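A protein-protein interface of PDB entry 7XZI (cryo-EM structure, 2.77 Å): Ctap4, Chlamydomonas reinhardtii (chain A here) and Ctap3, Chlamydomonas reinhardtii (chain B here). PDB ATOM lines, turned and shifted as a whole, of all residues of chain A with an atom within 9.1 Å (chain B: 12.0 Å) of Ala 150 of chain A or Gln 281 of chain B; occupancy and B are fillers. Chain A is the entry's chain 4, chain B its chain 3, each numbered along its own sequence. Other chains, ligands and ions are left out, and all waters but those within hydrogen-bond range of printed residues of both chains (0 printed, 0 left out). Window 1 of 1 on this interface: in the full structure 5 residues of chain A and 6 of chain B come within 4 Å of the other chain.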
ATOM      1  N   ALA A   3     -26.290  21.050 -20.802  1.00  0.00           N
ATOM      2  CA  ALA A   3     -27.108  22.215 -21.118  1.00  0.00           C
ATOM      3  C   ALA A   3     -28.298  22.317 -20.170  1.00  0.00           C
ATOM      4  O   ALA A   3     -28.914  21.310 -19.822  1.00  0.00           O
ATOM      5  CB  ALA A   3     -27.581  22.156 -22.561  1.00  0.00           C
ATOM      6  N   GLN A   5     -28.248  23.297 -16.983  1.00  0.00           N
ATOM      7  CA  GLN A   5     -27.856  22.751 -15.693  1.00  0.00           C
ATOM      8  C   GLN A   5     -27.169  23.831 -14.870  1.00  0.00           C
ATOM      9  O   GLN A   5     -26.621  24.798 -15.406  1.00  0.00           O
ATOM     10  CB  GLN A   5     -26.928  21.538 -15.852  1.00  0.00           C
ATOM     11  N   CYS A 140     -20.021  19.303 -27.482  1.00  0.00           N
ATOM     12  CA  CYS A 140     -20.908  18.920 -26.390  1.00  0.00           C
ATOM     13  C   CYS A 140     -21.462  17.525 -26.652  1.00  0.00           C
ATOM     14  O   CYS A 140     -22.013  17.264 -27.726  1.00  0.00           O
ATOM     15  CB  CYS A 140     -22.046  19.928 -26.233  1.00  0.00           C
ATOM     16  N   TRP A 141     -21.313  16.636 -25.673  1.00  0.00           N
ATOM     17  CA  TRP A 141     -21.888  15.297 -25.717  1.00  0.00           C
ATOM     18  C   TRP A 141     -22.890  15.168 -24.577  1.00  0.00           C
ATOM     19  O   TRP A 141     -22.534  15.358 -23.408  1.00  0.00           O
ATOM     20  CB  TRP A 141     -20.803  14.223 -25.610  1.00  0.00           C
ATOM     21  CG  TRP A 141     -19.845  14.197 -26.769  1.00  0.00           C
ATOM     22  CD1 TRP A 141     -19.938  14.915 -27.927  1.00  0.00           C
ATOM     23  CD2 TRP A 141     -18.650  13.413 -26.878  1.00  0.00           C
ATOM     24  NE1 TRP A 141     -18.875  14.626 -28.749  1.00  0.00           N
ATOM     25  CE2 TRP A 141     -18.070  13.708 -28.129  1.00  0.00           C
ATOM     26  CE3 TRP A 141     -18.014  12.491 -26.041  1.00  0.00           C
ATOM     27  CZ2 TRP A 141     -16.885  13.113 -28.562  1.00  0.00           C
ATOM     28  CZ3 TRP A 141     -16.838  11.903 -26.473  1.00  0.00           C
ATOM     29  CH2 TRP A 141     -16.287  12.216 -27.722  1.00  0.00           C
ATOM     30  N   THR A 142     -24.136  14.843 -24.914  1.00  0.00           N
ATOM     31  CA  THR A 142     -25.220  14.775 -23.941  1.00  0.00           C
ATOM     32  C   THR A 142     -25.878  13.404 -24.006  1.00  0.00           C
ATOM     33  O   THR A 142     -26.392  13.009 -25.059  1.00  0.00           O
ATOM     34  CB  THR A 142     -26.254  15.876 -24.191  1.00  0.00           C
ATOM     35  N   GLY A 143     -25.858  12.684 -22.885  1.00  0.00           N
ATOM     36  CA  GLY A 143     -26.568  11.425 -22.758  1.00  0.00           C
ATOM     37  C   GLY A 143     -27.078  11.194 -21.349  1.00  0.00           C
ATOM     38  O   GLY A 143     -26.303  11.258 -20.391  1.00  0.00           O
ATOM     39  N   GLU A 144     -28.373  10.924 -21.201  1.00  0.00           N
ATOM     40  CA  GLU A 144     -28.982  10.725 -19.892  1.00  0.00           C
ATOM     41  C   GLU A 144     -29.512   9.301 -19.769  1.00  0.00           C
ATOM     42  O   GLU A 144     -30.101   8.766 -20.714  1.00  0.00           O
ATOM     43  CB  GLU A 144     -30.101  11.742 -19.651  1.00  0.00           C
ATOM     44  CG  GLU A 144     -31.219  11.719 -20.679  1.00  0.00           C
ATOM     45  CD  GLU A 144     -32.440  10.959 -20.199  1.00  0.00           C
ATOM     46  OE1 GLU A 144     -32.386  10.367 -19.100  1.00  0.00           O
ATOM     47  OE2 GLU A 144     -33.458  10.960 -20.922  1.00  0.00           O
ATOM     48  N   ALA A 145     -29.281   8.686 -18.609  1.00  0.00           N
ATOM     49  CA  ALA A 145     -29.760   7.338 -18.314  1.00  0.00           C
ATOM     50  C   ALA A 145     -30.514   7.374 -16.993  1.00  0.00           C
ATOM     51  O   ALA A 145     -29.906   7.565 -15.933  1.00  0.00           O
ATOM     52  CB  ALA A 145     -28.606   6.337 -18.251  1.00  0.00           C
ATOM     53  N   GLY A 146     -31.827   7.178 -17.056  1.00  0.00           N
ATOM     54  CA  GLY A 146     -32.634   7.216 -15.847  1.00  0.00           C
ATOM     55  C   GLY A 146     -32.581   8.587 -15.207  1.00  0.00           C
ATOM     56  O   GLY A 146     -32.791   9.614 -15.862  1.00  0.00           O
ATOM     57  N   ALA A 147     -32.297   8.609 -13.905  1.00  0.00           N
ATOM     58  CA  ALA A 147     -32.175   9.874 -13.191  1.00  0.00           C
ATOM     59  C   ALA A 147     -30.902  10.625 -13.561  1.00  0.00           C
ATOM     60  O   ALA A 147     -30.904  11.861 -13.583  1.00  0.00           O
ATOM     61  N   ASP A 148     -29.819   9.910 -13.852  1.00  0.00           N
ATOM     62  CA  ASP A 148     -28.562  10.563 -14.192  1.00  0.00           C
ATOM     63  C   ASP A 148     -28.634  11.196 -15.576  1.00  0.00           C
ATOM     64  O   ASP A 148     -29.184  10.619 -16.517  1.00  0.00           O
ATOM     65  CB  ASP A 148     -27.408   9.562 -14.135  1.00  0.00           C
ATOM     66  CG  ASP A 148     -27.131   9.071 -12.730  1.00  0.00           C
ATOM     67  OD1 ASP A 148     -27.865   9.478 -11.805  1.00  0.00           O
ATOM     68  OD2 ASP A 148     -26.182   8.282 -12.548  1.00  0.00           O
ATOM     69  N   ARG A 149     -28.071  12.398 -15.691  1.00  0.00           N
ATOM     70  CA  ARG A 149     -27.970  13.104 -16.962  1.00  0.00           C
ATOM     71  C   ARG A 149     -26.546  13.616 -17.097  1.00  0.00           C
ATOM     72  O   ARG A 149     -26.094  14.417 -16.273  1.00  0.00           O
ATOM     73  CB  ARG A 149     -28.972  14.262 -17.039  1.00  0.00           C
ATOM     74  CG  ARG A 149     -28.928  15.036 -18.348  1.00  0.00           C
ATOM     75  N   ALA A 150     -25.846  13.163 -18.132  1.00  0.00           N
ATOM     76  CA  ALA A 150     -24.431  13.458 -18.315  1.00  0.00           C
ATOM     77  C   ALA A 150     -24.258  14.465 -19.442  1.00  0.00           C
ATOM     78  O   ALA A 150     -24.790  14.273 -20.540  1.00  0.00           O
ATOM     79  CB  ALA A 150     -23.638  12.184 -18.613  1.00  0.00           C
ATOM     80  N   THR A 151     -23.513  15.531 -19.164  1.00  0.00           N
ATOM     81  CA  THR A 151     -23.180  16.561 -20.148  1.00  0.00           C
ATOM     82  C   THR A 151     -21.669  16.768 -20.107  1.00  0.00           C
ATOM     83  O   THR A 151     -21.120  17.170 -19.076  1.00  0.00           O
ATOM     84  CB  THR A 151     -23.929  17.860 -19.863  1.00  0.00           C
ATOM     85  N   LEU A 152     -20.998  16.490 -21.221  1.00  0.00           N
ATOM     86  CA  LEU A 152     -19.552  16.638 -21.330  1.00  0.00           C
ATOM     87  C   LEU A 152     -19.242  17.720 -22.358  1.00  0.00           C
ATOM     88  O   LEU A 152     -19.700  17.643 -23.502  1.00  0.00           O
ATOM     89  CB  LEU A 152     -18.898  15.313 -21.722  1.00  0.00           C
ATOM     90  CG  LEU A 152     -17.390  15.337 -21.978  1.00  0.00           C
ATOM     91  CD1 LEU A 152     -16.635  15.779 -20.734  1.00  0.00           C
ATOM     92  CD2 LEU A 152     -16.907  13.973 -22.448  1.00  0.00           C
ATOM     93  N   LEU A 153     -18.467  18.723 -21.951  1.00  0.00           N
ATOM     94  CA  LEU A 153     -18.127  19.852 -22.807  1.00  0.00           C
ATOM     95  C   LEU A 153     -16.615  19.951 -22.949  1.00  0.00           C
ATOM     96  O   LEU A 153     -15.893  19.970 -21.946  1.00  0.00           O
ATOM     97  CB  LEU A 153     -18.694  21.158 -22.244  1.00  0.00           C
ATOM     98  N   ALA A 166     -15.390  19.985 -19.225  1.00  0.00           N
ATOM     99  CA  ALA A 166     -16.515  20.325 -18.366  1.00  0.00           C
ATOM    100  C   ALA A 166     -17.436  19.119 -18.272  1.00  0.00           C
ATOM    101  O   ALA A 166     -17.824  18.553 -19.298  1.00  0.00           O
ATOM    102  CB  ALA A 166     -17.279  21.541 -18.901  1.00  0.00           C
ATOM    103  N   ALA A 167     -17.778  18.732 -17.046  1.00  0.00           N
ATOM    104  CA  ALA A 167     -18.639  17.587 -16.794  1.00  0.00           C
ATOM    105  C   ALA A 167     -19.800  18.010 -15.908  1.00  0.00           C
ATOM    106  O   ALA A 167     -19.627  18.812 -14.986  1.00  0.00           O
ATOM    107  CB  ALA A 167     -17.867  16.441 -16.130  1.00  0.00           C
ATOM    108  N   ALA A 168     -20.983  17.472 -16.197  1.00  0.00           N
ATOM    109  CA  ALA A 168     -22.164  17.752 -15.392  1.00  0.00           C
ATOM    110  C   ALA A 168     -22.998  16.486 -15.271  1.00  0.00           C
ATOM    111  O   ALA A 168     -23.337  15.869 -16.285  1.00  0.00           O
ATOM    112  CB  ALA A 168     -22.997  18.883 -16.007  1.00  0.00           C
ATOM    113  N   VAL A 169     -23.323  16.107 -14.036  1.00  0.00           N
ATOM    114  CA  VAL A 169     -24.150  14.940 -13.751  1.00  0.00           C
ATOM    115  C   VAL A 169     -25.268  15.361 -12.808  1.00  0.00           C
ATOM    116  O   VAL A 169     -25.025  16.085 -11.836  1.00  0.00           O
ATOM    117  CB  VAL A 169     -23.329  13.783 -13.147  1.00  0.00           C
ATOM    118  CG1 VAL A 169     -22.482  13.120 -14.221  1.00  0.00           C
ATOM    119  CG2 VAL A 169     -22.448  14.284 -12.013  1.00  0.00           C
ATOM    120  N   ARG A 170     -26.488  14.914 -13.094  1.00  0.00           N
ATOM    121  CA  ARG A 170     -27.670  15.334 -12.354  1.00  0.00           C
ATOM    122  C   ARG A 170     -28.320  14.140 -11.670  1.00  0.00           C
ATOM    123  O   ARG A 170     -28.404  13.052 -12.246  1.00  0.00           O
ATOM    124  CB  ARG A 170     -28.684  16.018 -13.277  1.00  0.00           C
ATOM    125  N   THR A 171     -28.781  14.365 -10.441  1.00  0.00           N
ATOM    126  CA  THR A 171     -29.452  13.356  -9.628  1.00  0.00           C
ATOM    127  C   THR A 171     -28.681  12.033  -9.532  1.00  0.00           C
ATOM    128  O   THR A 171     -29.210  10.975  -9.874  1.00  0.00           O
ATOM    129  CB  THR A 171     -30.862  13.115 -10.154  1.00  0.00           C
ATOM    130  OG1 THR A 171     -31.397  14.351 -10.642  1.00  0.00           O
ATOM    131  CG2 THR A 171     -31.769  12.601  -9.045  1.00  0.00           C
ATOM    132  N   TYR A 201     -24.376  17.726  -8.462  1.00  0.00           N
ATOM    133  CA  TYR A 201     -23.576  18.182  -9.591  1.00  0.00           C
ATOM    134  C   TYR A 201     -22.093  18.128  -9.253  1.00  0.00           C
ATOM    135  O   TYR A 201     -21.666  18.555  -8.177  1.00  0.00           O
ATOM    136  CB  TYR A 201     -23.958  19.609  -9.983  1.00  0.00           C
ATOM    137  CG  TYR A 201     -25.395  19.780 -10.415  1.00  0.00           C
ATOM    138  CD1 TYR A 201     -25.917  19.043 -11.468  1.00  0.00           C
ATOM    139  CD2 TYR A 201     -26.223  20.697  -9.784  1.00  0.00           C
ATOM    140  CE1 TYR A 201     -27.231  19.203 -11.869  1.00  0.00           C
ATOM    141  CE2 TYR A 201     -27.534  20.865 -10.180  1.00  0.00           C
ATOM    142  CZ  TYR A 201     -28.033  20.117 -11.221  1.00  0.00           C
ATOM    143  OH  TYR A 201     -29.341  20.288 -11.611  1.00  0.00           O
ATOM    144  N   VAL A 202     -21.304  17.604 -10.186  1.00  0.00           N
ATOM    145  CA  VAL A 202     -19.851  17.577 -10.076  1.00  0.00           C
ATOM    146  C   VAL A 202     -19.276  18.192 -11.343  1.00  0.00           C
ATOM    147  O   VAL A 202     -19.491  17.670 -12.443  1.00  0.00           O
ATOM    148  CB  VAL A 202     -19.318  16.147  -9.867  1.00  0.00           C
ATOM    149  CG1 VAL A 202     -17.806  16.161  -9.727  1.00  0.00           C
ATOM    150  CG2 VAL A 202     -19.962  15.509  -8.644  1.00  0.00           C
ATOM    151  N   VAL B 272     -12.633   9.945  -9.587  1.00  0.00           N
ATOM    152  CA  VAL B 272     -14.008   9.576  -9.264  1.00  0.00           C
ATOM    153  C   VAL B 272     -14.986  10.330 -10.158  1.00  0.00           C
ATOM    154  O   VAL B 272     -15.931   9.745 -10.701  1.00  0.00           O
ATOM    155  CB  VAL B 272     -14.296   9.827  -7.772  1.00  0.00           C
ATOM    156  CG1 VAL B 272     -15.788   9.726  -7.493  1.00  0.00           C
ATOM    157  CG2 VAL B 272     -13.530   8.836  -6.911  1.00  0.00           C
ATOM    158  N   LEU B 273     -14.770  11.636 -10.328  1.00  0.00           N
ATOM    159  CA  LEU B 273     -15.666  12.432 -11.162  1.00  0.00           C
ATOM    160  C   LEU B 273     -15.634  11.971 -12.614  1.00  0.00           C
ATOM    161  O   LEU B 273     -16.684  11.836 -13.253  1.00  0.00           O
ATOM    162  CB  LEU B 273     -15.298  13.912 -11.062  1.00  0.00           C
ATOM    163  N   LYS B 274     -14.436  11.726 -13.151  1.00  0.00           N
ATOM    164  CA  LYS B 274     -14.320  11.286 -14.537  1.00  0.00           C
ATOM    165  C   LYS B 274     -14.971   9.923 -14.736  1.00  0.00           C
ATOM    166  O   LYS B 274     -15.673   9.697 -15.728  1.00  0.00           O
ATOM    167  CB  LYS B 274     -12.849  11.250 -14.953  1.00  0.00           C
ATOM    168  N   THR B 275     -14.744   8.996 -13.800  1.00  0.00           N
ATOM    169  CA  THR B 275     -15.349   7.673 -13.906  1.00  0.00           C
ATOM    170  C   THR B 275     -16.868   7.755 -13.831  1.00  0.00           C
ATOM    171  O   THR B 275     -17.570   7.089 -14.599  1.00  0.00           O
ATOM    172  CB  THR B 275     -14.806   6.758 -12.808  1.00  0.00           C
ATOM    173  OG1 THR B 275     -13.377   6.690 -12.905  1.00  0.00           O
ATOM    174  CG2 THR B 275     -15.380   5.357 -12.947  1.00  0.00           C
ATOM    175  N   LEU B 276     -17.395   8.574 -12.915  1.00  0.00           N
ATOM    176  CA  LEU B 276     -18.841   8.722 -12.798  1.00  0.00           C
ATOM    177  C   LEU B 276     -19.436   9.322 -14.066  1.00  0.00           C
ATOM    178  O   LEU B 276     -20.469   8.856 -14.561  1.00  0.00           O
ATOM    179  CB  LEU B 276     -19.181   9.583 -11.581  1.00  0.00           C
ATOM    180  CG  LEU B 276     -20.669   9.801 -11.299  1.00  0.00           C
ATOM    181  N   ASP B 277     -18.791  10.358 -14.611  1.00  0.00           N
ATOM    182  CA  ASP B 277     -19.293  10.979 -15.832  1.00  0.00           C
ATOM    183  C   ASP B 277     -19.252  10.009 -17.007  1.00  0.00           C
ATOM    184  O   ASP B 277     -20.208   9.931 -17.788  1.00  0.00           O
ATOM    185  CB  ASP B 277     -18.486  12.240 -16.146  1.00  0.00           C
ATOM    186  N   ARG B 278     -18.155   9.259 -17.145  1.00  0.00           N
ATOM    187  CA  ARG B 278     -18.042   8.301 -18.240  1.00  0.00           C
ATOM    188  C   ARG B 278     -19.071   7.184 -18.106  1.00  0.00           C
ATOM    189  O   ARG B 278     -19.658   6.752 -19.104  1.00  0.00           O
ATOM    190  CB  ARG B 278     -16.627   7.726 -18.291  1.00  0.00           C
ATOM    191  N   SER B 279     -19.294   6.695 -16.884  1.00  0.00           N
ATOM    192  CA  SER B 279     -20.298   5.658 -16.674  1.00  0.00           C
ATOM    193  C   SER B 279     -21.698   6.176 -16.972  1.00  0.00           C
ATOM    194  O   SER B 279     -22.518   5.465 -17.564  1.00  0.00           O
ATOM    195  CB  SER B 279     -20.213   5.126 -15.243  1.00  0.00           C
ATOM    196  N   ARG B 280     -21.997   7.412 -16.559  1.00  0.00           N
ATOM    197  CA  ARG B 280     -23.303   7.992 -16.851  1.00  0.00           C
ATOM    198  C   ARG B 280     -23.507   8.165 -18.351  1.00  0.00           C
ATOM    199  O   ARG B 280     -24.598   7.904 -18.871  1.00  0.00           O
ATOM    200  CB  ARG B 280     -23.457   9.331 -16.130  1.00  0.00           C
ATOM    201  N   GLN B 281     -22.470   8.615 -19.062  1.00  0.00           N
ATOM    202  CA  GLN B 281     -22.588   8.811 -20.503  1.00  0.00           C
ATOM    203  C   GLN B 281     -22.740   7.480 -21.232  1.00  0.00           C
ATOM    204  O   GLN B 281     -23.568   7.348 -22.141  1.00  0.00           O
ATOM    205  CB  GLN B 281     -21.371   9.577 -21.026  1.00  0.00           C
ATOM    206  N   LEU B 282     -21.940   6.481 -20.849  1.00  0.00           N
ATOM    207  CA  LEU B 282     -21.974   5.192 -21.534  1.00  0.00           C
ATOM    208  C   LEU B 282     -23.276   4.447 -21.265  1.00  0.00           C
ATOM    209  O   LEU B 282     -23.808   3.774 -22.155  1.00  0.00           O
ATOM    210  CB  LEU B 282     -20.776   4.343 -21.110  1.00  0.00           C
ATOM    211  N   GLU B 283     -23.798   4.545 -20.040  1.00  0.00           N
ATOM    212  CA  GLU B 283     -25.019   3.822 -19.695  1.00  0.00           C
ATOM    213  C   GLU B 283     -26.200   4.291 -20.536  1.00  0.00           C
ATOM    214  O   GLU B 283     -27.097   3.501 -20.854  1.00  0.00           O
ATOM    215  CB  GLU B 283     -25.326   3.986 -18.206  1.00  0.00           C
ATOM    216  N   TYR B 284     -26.221   5.576 -20.898  1.00  0.00           N
ATOM    217  CA  TYR B 284     -27.318   6.103 -21.704  1.00  0.00           C
ATOM    218  C   TYR B 284     -27.369   5.441 -23.073  1.00  0.00           C
ATOM    219  O   TYR B 284     -28.451   5.090 -23.561  1.00  0.00           O
ATOM    220  CB  TYR B 284     -27.179   7.618 -21.847  1.00  0.00           C
ATOM    221  N   ARG B 285     -26.214   5.254 -23.709  1.00  0.00           N
ATOM    222  CA  ARG B 285     -26.158   4.645 -25.038  1.00  0.00           C
ATOM    223  C   ARG B 285     -25.929   3.134 -24.932  1.00  0.00           C
ATOM    224  O   ARG B 285     -25.038   2.562 -25.554  1.00  0.00           O
ATOM    225  CB  ARG B 285     -25.074   5.312 -25.877  1.00  0.00           C
ATOM    226  N   LEU B 286     -26.767   2.480 -24.111  1.00  0.00           N
ATOM    227  CA  LEU B 286     -26.749   1.028 -23.969  1.00  0.00           C
ATOM    228  C   LEU B 286     -28.189   0.507 -23.880  1.00  0.00           C
ATOM    229  O   LEU B 286     -28.766   0.384 -22.799  1.00  0.00           O
ATOM    230  CB  LEU B 286     -25.921   0.598 -22.757  1.00  0.00           C
ATOM    231  N   ALA B 287     -28.763   0.175 -25.041  1.00  0.00           N
ATOM    232  CA  ALA B 287     -30.103  -0.411 -25.151  1.00  0.00           C
ATOM    233  C   ALA B 287     -31.168   0.420 -24.438  1.00  0.00           C
ATOM    234  O   ALA B 287     -32.220  -0.100 -24.051  1.00  0.00           O
ATOM    235  CB  ALA B 287     -30.122  -1.851 -24.629  1.00  0.00           C
ATOM    236  N   ARG B 288     -30.919   1.716 -24.267  1.00  0.00           N
ATOM    237  CA  ARG B 288     -31.846   2.601 -23.576  1.00  0.00           C
ATOM    238  C   ARG B 288     -32.626   3.500 -24.524  1.00  0.00           C
ATOM    239  O   ARG B 288     -33.168   4.520 -24.085  1.00  0.00           O
ATOM    240  CB  ARG B 288     -31.099   3.449 -22.544  1.00  0.00           C
ATOM    241  CG  ARG B 288     -30.728   2.695 -21.280  1.00  0.00           C
ATOM    242  CD  ARG B 288     -30.270   3.649 -20.191  1.00  0.00           C
ATOM    243  NE  ARG B 288     -29.989   2.956 -18.942  1.00  0.00           N
ATOM    244  N   MET B 289     -32.686   3.156 -25.813  1.00  0.00           N
ATOM    245  CA  MET B 289     -33.500   3.929 -26.746  1.00  0.00           C
ATOM    246  C   MET B 289     -34.969   3.896 -26.342  1.00  0.00           C
ATOM    247  O   MET B 289     -35.658   4.922 -26.387  1.00  0.00           O
ATOM    248  CB  MET B 289     -33.310   3.396 -28.165  1.00  0.00           C
ATOM    249  CG  MET B 289     -31.850   3.209 -28.547  1.00  0.00           C
ATOM    250  SD  MET B 289     -31.614   2.404 -30.142  1.00  0.00           S
ATOM    251  CE  MET B 289     -29.830   2.227 -30.166  1.00  0.00           C
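The backbone carbonyl oxygen of Gly 143 of chain A sits at hydrogen-bond distance from the backbone NH of Ala 150 of chain A (3.0 Å).
Among the printed residues, pairs that only touch across the chains: Gly 143 of chain A with Tyr 284 of chain B, Glu 144 of chain A with Tyr 284 of chain B, Ala 145 of chain A with Glu 283 of chain B, Ala 145 of chain A with Tyr 284 of chain B, Ala 145 of chain A with Arg 288 of chain B, Ala 150 of chain A with Arg 280 of chain B, Ala 150 of chain A with Gln 281 of chain B and Val 202 of chain A with Leu 273 of chain B.
Of chain B, only Arg 280 (3.8 Å) and Gln 281 (3.8 Å) come within 4 Å of Ala 150 of chain A. Gln 281 of chain B touches just one residue of chain A: Ala 150. No residue of chain B comes within 4 Å of Thr 142 of chain A. Ala 145 of chain A touches just these residues of chain B: Glu 283, Tyr 284 and Arg 288. No residue of chain B comes within 4 Å of Asp 148 of chain A. No residue of chain B comes within 4 Å of Arg 149 of chain A. No residue of chain B comes within 4 Å of Thr 151 of chain A. No residue of chain B comes within 4 Å of Ala 168 of chain A. No residue of chain B comes within 4 Å of Arg 170 of chain A. Of chain A, only Ala 150 (3.8 Å) comes within 4 Å of Arg 280 of chain B. No residue of chain A comes within 4 Å of Leu 282 of chain B. Of the printed residues of chain B, Val 202 of chain A touches Leu 273 (3.6 Å). Printed residues of chain A within 4 Å of Leu 273 of chain B: Val 202. Of the printed residues of chain A, Tyr 284 of chain B touches Gly 143, Glu 144 and Ala 145. Of the printed residues of chain B, Glu 144 of chain A touches Tyr 284 (3.3 Å). Trp 141 of chain A touches none of the printed residues of chain B. Ala 167 of chain A touches none of the printed residues of chain B. The nearest residue of chain B that does not touch Ala 150 of chain A is Asp 277 of chain B (4.2 Å). The nearest printed residue of chain A that does not touch Arg 288 of chain B is Gly 146 of chain A (5.0 Å).
Hydrophobic or aromatic side chains of chain A that line the printed part of chain B: Ala 145, Ala 150 and Val 202. Hydrophobic or aromatic side chains of chain B within 4 Å of the printed part of chain A: Leu 273 and Tyr 284. Among the printed residues, 8 pairs touch across the chains.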
